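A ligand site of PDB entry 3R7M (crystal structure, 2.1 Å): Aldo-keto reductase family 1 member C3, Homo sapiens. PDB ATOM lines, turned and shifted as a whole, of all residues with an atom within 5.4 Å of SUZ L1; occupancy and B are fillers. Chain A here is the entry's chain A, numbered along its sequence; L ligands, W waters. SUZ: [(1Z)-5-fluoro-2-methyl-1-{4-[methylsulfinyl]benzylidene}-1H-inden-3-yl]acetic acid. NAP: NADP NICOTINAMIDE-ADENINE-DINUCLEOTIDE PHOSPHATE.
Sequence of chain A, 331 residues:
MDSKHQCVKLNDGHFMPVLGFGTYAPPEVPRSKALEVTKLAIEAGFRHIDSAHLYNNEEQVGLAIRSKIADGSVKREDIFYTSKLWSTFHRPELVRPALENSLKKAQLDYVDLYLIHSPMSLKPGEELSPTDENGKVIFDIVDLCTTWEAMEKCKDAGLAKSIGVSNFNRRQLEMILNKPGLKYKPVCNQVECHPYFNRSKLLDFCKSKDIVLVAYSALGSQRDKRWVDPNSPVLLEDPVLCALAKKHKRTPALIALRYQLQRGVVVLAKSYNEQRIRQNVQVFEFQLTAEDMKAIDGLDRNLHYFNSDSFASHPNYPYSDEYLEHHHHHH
The side-chain amide nitrogen (ND2) of Asn 167 sits close to a fluorine (F) of SUZ L1 (2.8 Å).
Residues that only touch SUZ L1: Trp 227, Leu 54, Tyr 24, Phe 311, Trp 86, Ser 118 and Phe 306.
Hydrophobic or aromatic side chains within 4 Å of SUZ L1: Tyr 24, Leu 54, Tyr 55, Trp 86, His 117, Trp 227, Phe 306 and Phe 311.
Within 4 Å of SUZ L1: Tyr 24, Leu 54, Tyr 55, Trp 86, His 117, Ser 118, Asn 167, Trp 227, Phe 306 and Phe 311.
An oxygen (O3) of SUZ L1 sits at hydrogen-bond distance from the side-chain hydroxyl (OH) of Tyr 55, 2.5 Å away.
A ring nitrogen (NE2) of His 117 lies within hydrogen-bond range of an oxygen (O3) of SUZ L1 (3.0 Å).
ND2 of Asn 167 is in hydrogen-bond range of O7N of NAP L2, at 2.9 Å.
An oxygen (O3D) of NAP L2 lies within hydrogen-bond range of the backbone NH (N) of Tyr 24 (3.3 Å).
The side-chain hydroxyl (OH) of Tyr 55 is in hydrogen-bond range of the side-chain amino group (NZ) of Lys 84.
The backbone carbonyl oxygen (O) of His 117 lies within hydrogen-bond range of the side-chain amide nitrogen (ND2) of Asn 167 (2.9 Å).
OH of Tyr 216 sits at hydrogen-bond distance from OD1 of Asn 167, at 2.5 Å.
The side-chain hydroxyl (OH) of Tyr 24 is in hydrogen-bond range of the guanidinium group (NH2) of Arg 226 (3.0 Å).
The side-chain hydroxyl (OG) of Ser 118 sits at hydrogen-bond distance from the backbone NH (N) of Met 120.
Water W1 bridges an oxygen (O2) of SUZ L1 (2.8 Å) and an oxygen (O1N) of NAP L2 (3.1 Å).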
ATOM      1  N   TYR A  24      30.878  -8.768 -30.380  1.00  0.00           N
ATOM      2  CA  TYR A  24      30.191  -7.576 -30.803  1.00  0.00           C
ATOM      3  C   TYR A  24      30.759  -7.053 -32.097  1.00  0.00           C
ATOM      4  O   TYR A  24      31.990  -6.897 -32.235  1.00  0.00           O
ATOM      5  CB  TYR A  24      30.201  -6.419 -29.787  1.00  0.00           C
ATOM      6  CG  TYR A  24      29.429  -5.225 -30.339  1.00  0.00           C
ATOM      7  CD1 TYR A  24      28.037  -5.247 -30.353  1.00  0.00           C
ATOM      8  CD2 TYR A  24      30.062  -4.095 -30.850  1.00  0.00           C
ATOM      9  CE1 TYR A  24      27.274  -4.180 -30.864  1.00  0.00           C
ATOM     10  CE2 TYR A  24      29.324  -2.996 -31.355  1.00  0.00           C
ATOM     11  CZ  TYR A  24      27.940  -3.052 -31.351  1.00  0.00           C
ATOM     12  OH  TYR A  24      27.175  -2.011 -31.844  1.00  0.00           O
ATOM     13  N   LEU A  54      22.146  -7.269 -26.231  1.00  0.00           N
ATOM     14  CA  LEU A  54      22.408  -6.025 -26.962  1.00  0.00           C
ATOM     15  C   LEU A  54      23.024  -6.255 -28.341  1.00  0.00           C
ATOM     16  O   LEU A  54      22.778  -5.468 -29.276  1.00  0.00           O
ATOM     17  CB  LEU A  54      23.248  -5.037 -26.156  1.00  0.00           C
ATOM     18  CG  LEU A  54      23.628  -3.722 -26.873  1.00  0.00           C
ATOM     19  CD1 LEU A  54      22.425  -2.715 -27.006  1.00  0.00           C
ATOM     20  CD2 LEU A  54      24.763  -3.083 -26.122  1.00  0.00           C
ATOM     21  N   TYR A  55      23.783  -7.336 -28.488  1.00  0.00           N
ATOM     22  CA  TYR A  55      24.629  -7.482 -29.710  1.00  0.00           C
ATOM     23  C   TYR A  55      23.857  -7.886 -30.955  1.00  0.00           C
ATOM     24  O   TYR A  55      24.420  -7.782 -32.076  1.00  0.00           O
ATOM     25  CB  TYR A  55      25.816  -8.438 -29.474  1.00  0.00           C
ATOM     26  CG  TYR A  55      26.682  -8.018 -28.310  1.00  0.00           C
ATOM     27  CD1 TYR A  55      26.597  -6.710 -27.772  1.00  0.00           C
ATOM     28  CD2 TYR A  55      27.590  -8.907 -27.728  1.00  0.00           C
ATOM     29  CE1 TYR A  55      27.417  -6.316 -26.634  1.00  0.00           C
ATOM     30  CE2 TYR A  55      28.396  -8.533 -26.621  1.00  0.00           C
ATOM     31  CZ  TYR A  55      28.321  -7.235 -26.107  1.00  0.00           C
ATOM     32  OH  TYR A  55      29.086  -6.880 -24.993  1.00  0.00           O
ATOM     33  N   LYS A  84      24.174 -11.466 -21.598  1.00  0.00           N
ATOM     34  CA  LYS A  84      24.030 -10.349 -20.649  1.00  0.00           C
ATOM     35  C   LYS A  84      22.645  -9.794 -20.696  1.00  0.00           C
ATOM     36  O   LYS A  84      22.019  -9.634 -21.800  1.00  0.00           O
ATOM     37  CB  LYS A  84      24.998  -9.205 -20.945  1.00  0.00           C
ATOM     38  CG  LYS A  84      26.498  -9.653 -21.190  1.00  0.00           C
ATOM     39  CD  LYS A  84      27.423  -8.445 -21.275  1.00  0.00           C
ATOM     40  CE  LYS A  84      28.882  -8.896 -21.769  1.00  0.00           C
ATOM     41  NZ  LYS A  84      28.897  -9.178 -23.225  1.00  0.00           N
ATOM     42  N   TRP A  86      20.132  -6.880 -20.700  1.00  0.00           N
ATOM     43  CA  TRP A  86      20.185  -5.516 -21.126  1.00  0.00           C
ATOM     44  C   TRP A  86      19.462  -4.602 -20.090  1.00  0.00           C
ATOM     45  O   TRP A  86      18.619  -5.058 -19.325  1.00  0.00           O
ATOM     46  CB  TRP A  86      19.637  -5.392 -22.577  1.00  0.00           C
ATOM     47  CG  TRP A  86      19.649  -3.978 -23.043  1.00  0.00           C
ATOM     48  CD1 TRP A  86      18.576  -3.217 -23.437  1.00  0.00           C
ATOM     49  CD2 TRP A  86      20.789  -3.091 -23.072  1.00  0.00           C
ATOM     50  NE1 TRP A  86      18.960  -1.927 -23.703  1.00  0.00           N
ATOM     51  CE2 TRP A  86      20.306  -1.808 -23.485  1.00  0.00           C
ATOM     52  CE3 TRP A  86      22.138  -3.230 -22.752  1.00  0.00           C
ATOM     53  CZ2 TRP A  86      21.172  -0.701 -23.669  1.00  0.00           C
ATOM     54  CZ3 TRP A  86      23.007  -2.107 -22.884  1.00  0.00           C
ATOM     55  CH2 TRP A  86      22.496  -0.849 -23.331  1.00  0.00           C
ATOM     56  N   HIS A 117      24.438  -6.259 -17.622  1.00  0.00           N
ATOM     57  CA  HIS A 117      25.322  -5.701 -18.652  1.00  0.00           C
ATOM     58  C   HIS A 117      25.883  -4.356 -18.176  1.00  0.00           C
ATOM     59  O   HIS A 117      27.046  -3.958 -18.503  1.00  0.00           O
ATOM     60  CB  HIS A 117      24.534  -5.513 -19.954  1.00  0.00           C
ATOM     61  CG  HIS A 117      25.393  -5.318 -21.173  1.00  0.00           C
ATOM     62  ND1 HIS A 117      24.980  -5.685 -22.433  1.00  0.00           N
ATOM     63  CD2 HIS A 117      26.600  -4.707 -21.339  1.00  0.00           C
ATOM     64  CE1 HIS A 117      25.923  -5.381 -23.314  1.00  0.00           C
ATOM     65  NE2 HIS A 117      26.904  -4.772 -22.676  1.00  0.00           N
ATOM     66  N   SER A 118      25.083  -3.665 -17.370  1.00  0.00           N
ATOM     67  CA  SER A 118      25.448  -2.355 -16.933  1.00  0.00           C
ATOM     68  C   SER A 118      24.574  -1.958 -15.771  1.00  0.00           C
ATOM     69  O   SER A 118      23.429  -2.399 -15.708  1.00  0.00           O
ATOM     70  CB  SER A 118      25.241  -1.398 -18.113  1.00  0.00           C
ATOM     71  OG  SER A 118      25.055  -0.051 -17.694  1.00  0.00           O
ATOM     72  N   MET A 120      23.393   0.992 -15.444  1.00  0.00           N
ATOM     73  CA  MET A 120      22.688   2.210 -15.786  1.00  0.00           C
ATOM     74  C   MET A 120      21.324   1.905 -16.324  1.00  0.00           C
ATOM     75  O   MET A 120      21.171   1.774 -17.502  1.00  0.00           O
ATOM     76  CB  MET A 120      23.507   3.032 -16.790  1.00  0.00           C
ATOM     77  CG  MET A 120      24.739   3.688 -16.161  1.00  0.00           C
ATOM     78  SD  MET A 120      25.766   4.472 -17.446  1.00  0.00           S
ATOM     79  CE  MET A 120      26.449   2.947 -18.193  1.00  0.00           C
ATOM     80  N   LEU A 122      17.534   1.624 -17.762  1.00  0.00           N
ATOM     81  CA  LEU A 122      16.742   2.289 -18.820  1.00  0.00           C
ATOM     82  C   LEU A 122      15.246   1.928 -18.680  1.00  0.00           C
ATOM     83  O   LEU A 122      14.925   0.822 -18.165  1.00  0.00           O
ATOM     84  CB  LEU A 122      17.234   1.865 -20.180  1.00  0.00           C
ATOM     85  CG  LEU A 122      18.717   2.158 -20.463  1.00  0.00           C
ATOM     86  CD1 LEU A 122      19.050   1.791 -21.900  1.00  0.00           C
ATOM     87  CD2 LEU A 122      19.097   3.646 -20.136  1.00  0.00           C
ATOM     88  N   ASN A 167      30.534  -3.609 -15.769  1.00  0.00           N
ATOM     89  CA  ASN A 167      30.579  -2.156 -15.632  1.00  0.00           C
ATOM     90  C   ASN A 167      30.232  -1.635 -14.224  1.00  0.00           C
ATOM     91  O   ASN A 167      29.803  -0.495 -14.081  1.00  0.00           O
ATOM     92  CB  ASN A 167      29.649  -1.473 -16.700  1.00  0.00           C
ATOM     93  CG  ASN A 167      30.164  -1.673 -18.128  1.00  0.00           C
ATOM     94  OD1 ASN A 167      31.313  -1.293 -18.461  1.00  0.00           O
ATOM     95  ND2 ASN A 167      29.326  -2.242 -18.976  1.00  0.00           N
ATOM     96  N   TYR A 216      37.291  -6.107 -21.036  1.00  0.00           N
ATOM     97  CA  TYR A 216      36.873  -5.801 -22.424  1.00  0.00           C
ATOM     98  C   TYR A 216      37.605  -4.544 -22.938  1.00  0.00           C
ATOM     99  O   TYR A 216      38.237  -3.826 -22.126  1.00  0.00           O
ATOM    100  CB  TYR A 216      35.343  -5.658 -22.519  1.00  0.00           C
ATOM    101  CG  TYR A 216      34.706  -4.381 -21.954  1.00  0.00           C
ATOM    102  CD1 TYR A 216      34.949  -3.147 -22.540  1.00  0.00           C
ATOM    103  CD2 TYR A 216      33.853  -4.445 -20.862  1.00  0.00           C
ATOM    104  CE1 TYR A 216      34.327  -1.991 -22.058  1.00  0.00           C
ATOM    105  CE2 TYR A 216      33.210  -3.295 -20.378  1.00  0.00           C
ATOM    106  CZ  TYR A 216      33.450  -2.088 -20.971  1.00  0.00           C
ATOM    107  OH  TYR A 216      32.832  -0.962 -20.458  1.00  0.00           O
ATOM    108  N   ARG A 226      30.266   6.587 -32.240  1.00  0.00           N
ATOM    109  CA  ARG A 226      29.145   6.910 -31.362  1.00  0.00           C
ATOM    110  C   ARG A 226      29.567   7.017 -29.898  1.00  0.00           C
ATOM    111  O   ARG A 226      28.908   7.726 -29.145  1.00  0.00           O
ATOM    112  CB  ARG A 226      28.005   5.901 -31.497  1.00  0.00           C
ATOM    113  CG  ARG A 226      27.493   5.700 -32.986  1.00  0.00           C
ATOM    114  CD  ARG A 226      26.583   4.457 -33.103  1.00  0.00           C
ATOM    115  NE  ARG A 226      27.300   3.171 -33.199  1.00  0.00           N
ATOM    116  CZ  ARG A 226      26.796   2.011 -32.742  1.00  0.00           C
ATOM    117  NH1 ARG A 226      25.594   2.021 -32.174  1.00  0.00           N
ATOM    118  NH2 ARG A 226      27.493   0.851 -32.833  1.00  0.00           N
ATOM    119  N   TRP A 227      30.671   6.388 -29.488  1.00  0.00           N
ATOM    120  CA  TRP A 227      31.048   6.483 -28.046  1.00  0.00           C
ATOM    121  C   TRP A 227      32.508   6.752 -27.775  1.00  0.00           C
ATOM    122  O   TRP A 227      32.900   6.995 -26.629  1.00  0.00           O
ATOM    123  CB  TRP A 227      30.701   5.209 -27.332  1.00  0.00           C
ATOM    124  CG  TRP A 227      29.424   4.792 -27.684  1.00  0.00           C
ATOM    125  CD1 TRP A 227      28.203   5.465 -27.411  1.00  0.00           C
ATOM    126  CD2 TRP A 227      29.112   3.657 -28.428  1.00  0.00           C
ATOM    127  NE1 TRP A 227      27.176   4.752 -27.960  1.00  0.00           N
ATOM    128  CE2 TRP A 227      27.696   3.634 -28.585  1.00  0.00           C
ATOM    129  CE3 TRP A 227      29.879   2.620 -28.954  1.00  0.00           C
ATOM    130  CZ2 TRP A 227      27.044   2.627 -29.276  1.00  0.00           C
ATOM    131  CZ3 TRP A 227      29.237   1.626 -29.646  1.00  0.00           C
ATOM    132  CH2 TRP A 227      27.824   1.631 -29.797  1.00  0.00           C
ATOM    133  N   PHE A 306      35.146   4.362 -24.006  1.00  0.00           N
ATOM    134  CA  PHE A 306      33.726   4.674 -24.032  1.00  0.00           C
ATOM    135  C   PHE A 306      33.530   5.917 -23.193  1.00  0.00           C
ATOM    136  O   PHE A 306      33.718   5.887 -21.964  1.00  0.00           O
ATOM    137  CB  PHE A 306      32.935   3.528 -23.434  1.00  0.00           C
ATOM    138  CG  PHE A 306      32.860   2.312 -24.354  1.00  0.00           C
ATOM    139  CD1 PHE A 306      31.722   2.119 -25.137  1.00  0.00           C
ATOM    140  CD2 PHE A 306      33.903   1.404 -24.441  1.00  0.00           C
ATOM    141  CE1 PHE A 306      31.593   1.022 -26.007  1.00  0.00           C
ATOM    142  CE2 PHE A 306      33.788   0.231 -25.306  1.00  0.00           C
ATOM    143  CZ  PHE A 306      32.623   0.072 -26.099  1.00  0.00           C
ATOM    144  N   SER A 310      25.798   9.688 -23.408  1.00  0.00           N
ATOM    145  CA  SER A 310      24.758   8.647 -23.170  1.00  0.00           C
ATOM    146  C   SER A 310      24.988   7.887 -21.872  1.00  0.00           C
ATOM    147  O   SER A 310      24.065   7.344 -21.321  1.00  0.00           O
ATOM    148  CB  SER A 310      24.726   7.576 -24.232  1.00  0.00           C
ATOM    149  OG  SER A 310      24.715   8.172 -25.463  1.00  0.00           O
ATOM    150  N   PHE A 311      26.225   7.862 -21.393  1.00  0.00           N
ATOM    151  CA  PHE A 311      26.490   7.121 -20.162  1.00  0.00           C
ATOM    152  C   PHE A 311      26.731   8.163 -19.079  1.00  0.00           C
ATOM    153  O   PHE A 311      26.284   7.999 -17.974  1.00  0.00           O
ATOM    154  CB  PHE A 311      27.792   6.279 -20.312  1.00  0.00           C
ATOM    155  CG  PHE A 311      27.789   5.380 -21.500  1.00  0.00           C
ATOM    156  CD1 PHE A 311      26.729   4.450 -21.698  1.00  0.00           C
ATOM    157  CD2 PHE A 311      28.811   5.471 -22.446  1.00  0.00           C
ATOM    158  CE1 PHE A 311      26.717   3.600 -22.835  1.00  0.00           C
ATOM    159  CE2 PHE A 311      28.809   4.634 -23.585  1.00  0.00           C
ATOM    160  CZ  PHE A 311      27.761   3.674 -23.782  1.00  0.00           C
HETATM  161  C20 SUZ L   1      22.382   1.843 -26.202  1.00  0.00           C
HETATM  162  C19 SUZ L   1      23.351   0.954 -26.677  1.00  0.00           C
HETATM  163  C5  SUZ L   1      24.705   1.277 -26.558  1.00  0.00           C
HETATM  164  C6  SUZ L   1      25.686   0.426 -27.076  1.00  0.00           C
HETATM  165  C7  SUZ L   1      26.637  -0.227 -26.244  1.00  0.00           C
HETATM  166  C18 SUZ L   1      26.697  -0.335 -24.839  1.00  0.00           C
HETATM  167  C17 SUZ L   1      25.931   0.210 -23.799  1.00  0.00           C
HETATM  168  C16 SUZ L   1      26.258  -0.088 -22.463  1.00  0.00           C
HETATM  169  C15 SUZ L   1      27.322  -0.924 -22.182  1.00  0.00           C
HETATM  170  F   SUZ L   1      27.650  -1.199 -20.912  1.00  0.00           F
HETATM  171  C14 SUZ L   1      28.103  -1.472 -23.214  1.00  0.00           C
HETATM  172  C13 SUZ L   1      27.797  -1.181 -24.530  1.00  0.00           C
HETATM  173  C10 SUZ L   1      28.399  -1.620 -25.728  1.00  0.00           C
HETATM  174  C11 SUZ L   1      29.675  -2.436 -25.883  1.00  0.00           C
HETATM  175  C12 SUZ L   1      29.607  -3.946 -25.767  1.00  0.00           C
HETATM  176  O3  SUZ L   1      28.896  -4.434 -24.864  1.00  0.00           O
HETATM  177  O2  SUZ L   1      30.347  -4.576 -26.584  1.00  0.00           O
HETATM  178  C8  SUZ L   1      27.682  -1.018 -26.767  1.00  0.00           C
HETATM  179  C9  SUZ L   1      28.025  -1.223 -28.277  1.00  0.00           C
HETATM  180  C4  SUZ L   1      25.071   2.522 -26.026  1.00  0.00           C
HETATM  181  C3  SUZ L   1      24.119   3.399 -25.539  1.00  0.00           C
HETATM  182  C2  SUZ L   1      22.761   3.058 -25.645  1.00  0.00           C
HETATM  183  S   SUZ L   1      21.499   4.164 -25.017  1.00  0.00           S
HETATM  184  O1  SUZ L   1      21.908   4.519 -23.604  1.00  0.00           O
HETATM  185  C1  SUZ L   1      21.398   5.574 -26.093  1.00  0.00           C
HETATM  186  PA  NAP L   2      38.698  -5.310 -28.632  1.00  0.00           P
HETATM  187  O1A NAP L   2      38.739  -6.616 -28.031  1.00  0.00           O
HETATM  188  O2A NAP L   2      39.345  -4.188 -27.744  1.00  0.00           O
HETATM  189  O5B NAP L   2      39.362  -5.190 -30.120  1.00  0.00           O
HETATM  190  C5B NAP L   2      39.561  -3.851 -30.728  1.00  0.00           C
HETATM  191  C4B NAP L   2      39.888  -4.112 -32.271  1.00  0.00           C
HETATM  192  O4B NAP L   2      41.086  -4.951 -32.104  1.00  0.00           O
HETATM  193  C3B NAP L   2      38.942  -5.103 -32.857  1.00  0.00           C
HETATM  194  O3B NAP L   2      37.880  -4.489 -33.598  1.00  0.00           O
HETATM  195  C2B NAP L   2      39.874  -5.927 -33.781  1.00  0.00           C
HETATM  196  O2B NAP L   2      39.736  -5.549 -35.209  1.00  0.00           O
HETATM  197  C1B NAP L   2      41.250  -5.532 -33.385  1.00  0.00           C
HETATM  198  N9A NAP L   2      42.093  -6.784 -33.216  1.00  0.00           N
HETATM  199  C8A NAP L   2      41.728  -8.009 -32.770  1.00  0.00           C
HETATM  200  N7A NAP L   2      42.819  -8.770 -32.757  1.00  0.00           N
HETATM  201  C5A NAP L   2      43.831  -8.040 -33.216  1.00  0.00           C
HETATM  202  C6A NAP L   2      45.172  -8.336 -33.471  1.00  0.00           C
HETATM  203  N6A NAP L   2      45.707  -9.567 -33.181  1.00  0.00           N
HETATM  204  N1A NAP L   2      45.946  -7.334 -33.940  1.00  0.00           N
HETATM  205  C2A NAP L   2      45.461  -6.085 -34.240  1.00  0.00           C
HETATM  206  N3A NAP L   2      44.179  -5.771 -34.025  1.00  0.00           N
HETATM  207  C4A NAP L   2      43.373  -6.766 -33.505  1.00  0.00           C
HETATM  208  O3  NAP L   2      37.139  -4.988 -28.881  1.00  0.00           O
HETATM  209  PN  NAP L   2      35.861  -4.580 -28.008  1.00  0.00           P
HETATM  210  O1N NAP L   2      34.775  -5.021 -28.912  1.00  0.00           O
HETATM  211  O2N NAP L   2      35.869  -3.206 -27.391  1.00  0.00           O
HETATM  212  O5D NAP L   2      36.015  -5.707 -26.730  1.00  0.00           O
HETATM  213  C5D NAP L   2      35.869  -7.145 -27.009  1.00  0.00           C
HETATM  214  C4D NAP L   2      34.530  -7.742 -26.494  1.00  0.00           C
HETATM  215  O4D NAP L   2      34.297  -7.364 -25.125  1.00  0.00           O
HETATM  216  C3D NAP L   2      33.377  -7.009 -27.077  1.00  0.00           C
HETATM  217  O3D NAP L   2      33.249  -7.530 -28.412  1.00  0.00           O
HETATM  218  C2D NAP L   2      32.213  -7.592 -26.333  1.00  0.00           C
HETATM  219  O2D NAP L   2      32.168  -9.036 -26.540  1.00  0.00           O
HETATM  220  C1D NAP L   2      32.814  -7.325 -24.981  1.00  0.00           C
HETATM  221  N1N NAP L   2      32.608  -5.935 -24.581  1.00  0.00           N
HETATM  222  C2N NAP L   2      31.707  -5.796 -23.520  1.00  0.00           C
HETATM  223  C3N NAP L   2      31.426  -4.524 -23.045  1.00  0.00           C
HETATM  224  C7N NAP L   2      30.499  -4.425 -21.830  1.00  0.00           C
HETATM  225  O7N NAP L   2      29.963  -3.340 -21.586  1.00  0.00           O
HETATM  226  N7N NAP L   2      30.462  -5.512 -20.975  1.00  0.00           N
HETATM  227  C4N NAP L   2      31.987  -3.374 -23.638  1.00  0.00           C
HETATM  228  C5N NAP L   2      32.878  -3.515 -24.718  1.00  0.00           C
HETATM  229  C6N NAP L   2      33.195  -4.799 -25.189  1.00  0.00           C
HETATM  230  P2B NAP L   2      39.306  -6.743 -36.270  1.00  0.00           P
HETATM  231  O1X NAP L   2      37.894  -7.259 -36.068  1.00  0.00           O
HETATM  232  O2X NAP L   2      39.547  -5.928 -37.623  1.00  0.00           O
HETATM  233  O3X NAP L   2      40.481  -7.844 -36.126  1.00  0.00           O
HETATM  234  O   HOH W   1      32.188  -3.353 -28.300  1.00  0.00           O
HETATM  235  O   HOH W   2      23.162   2.783 -21.157  1.00  0.00           O
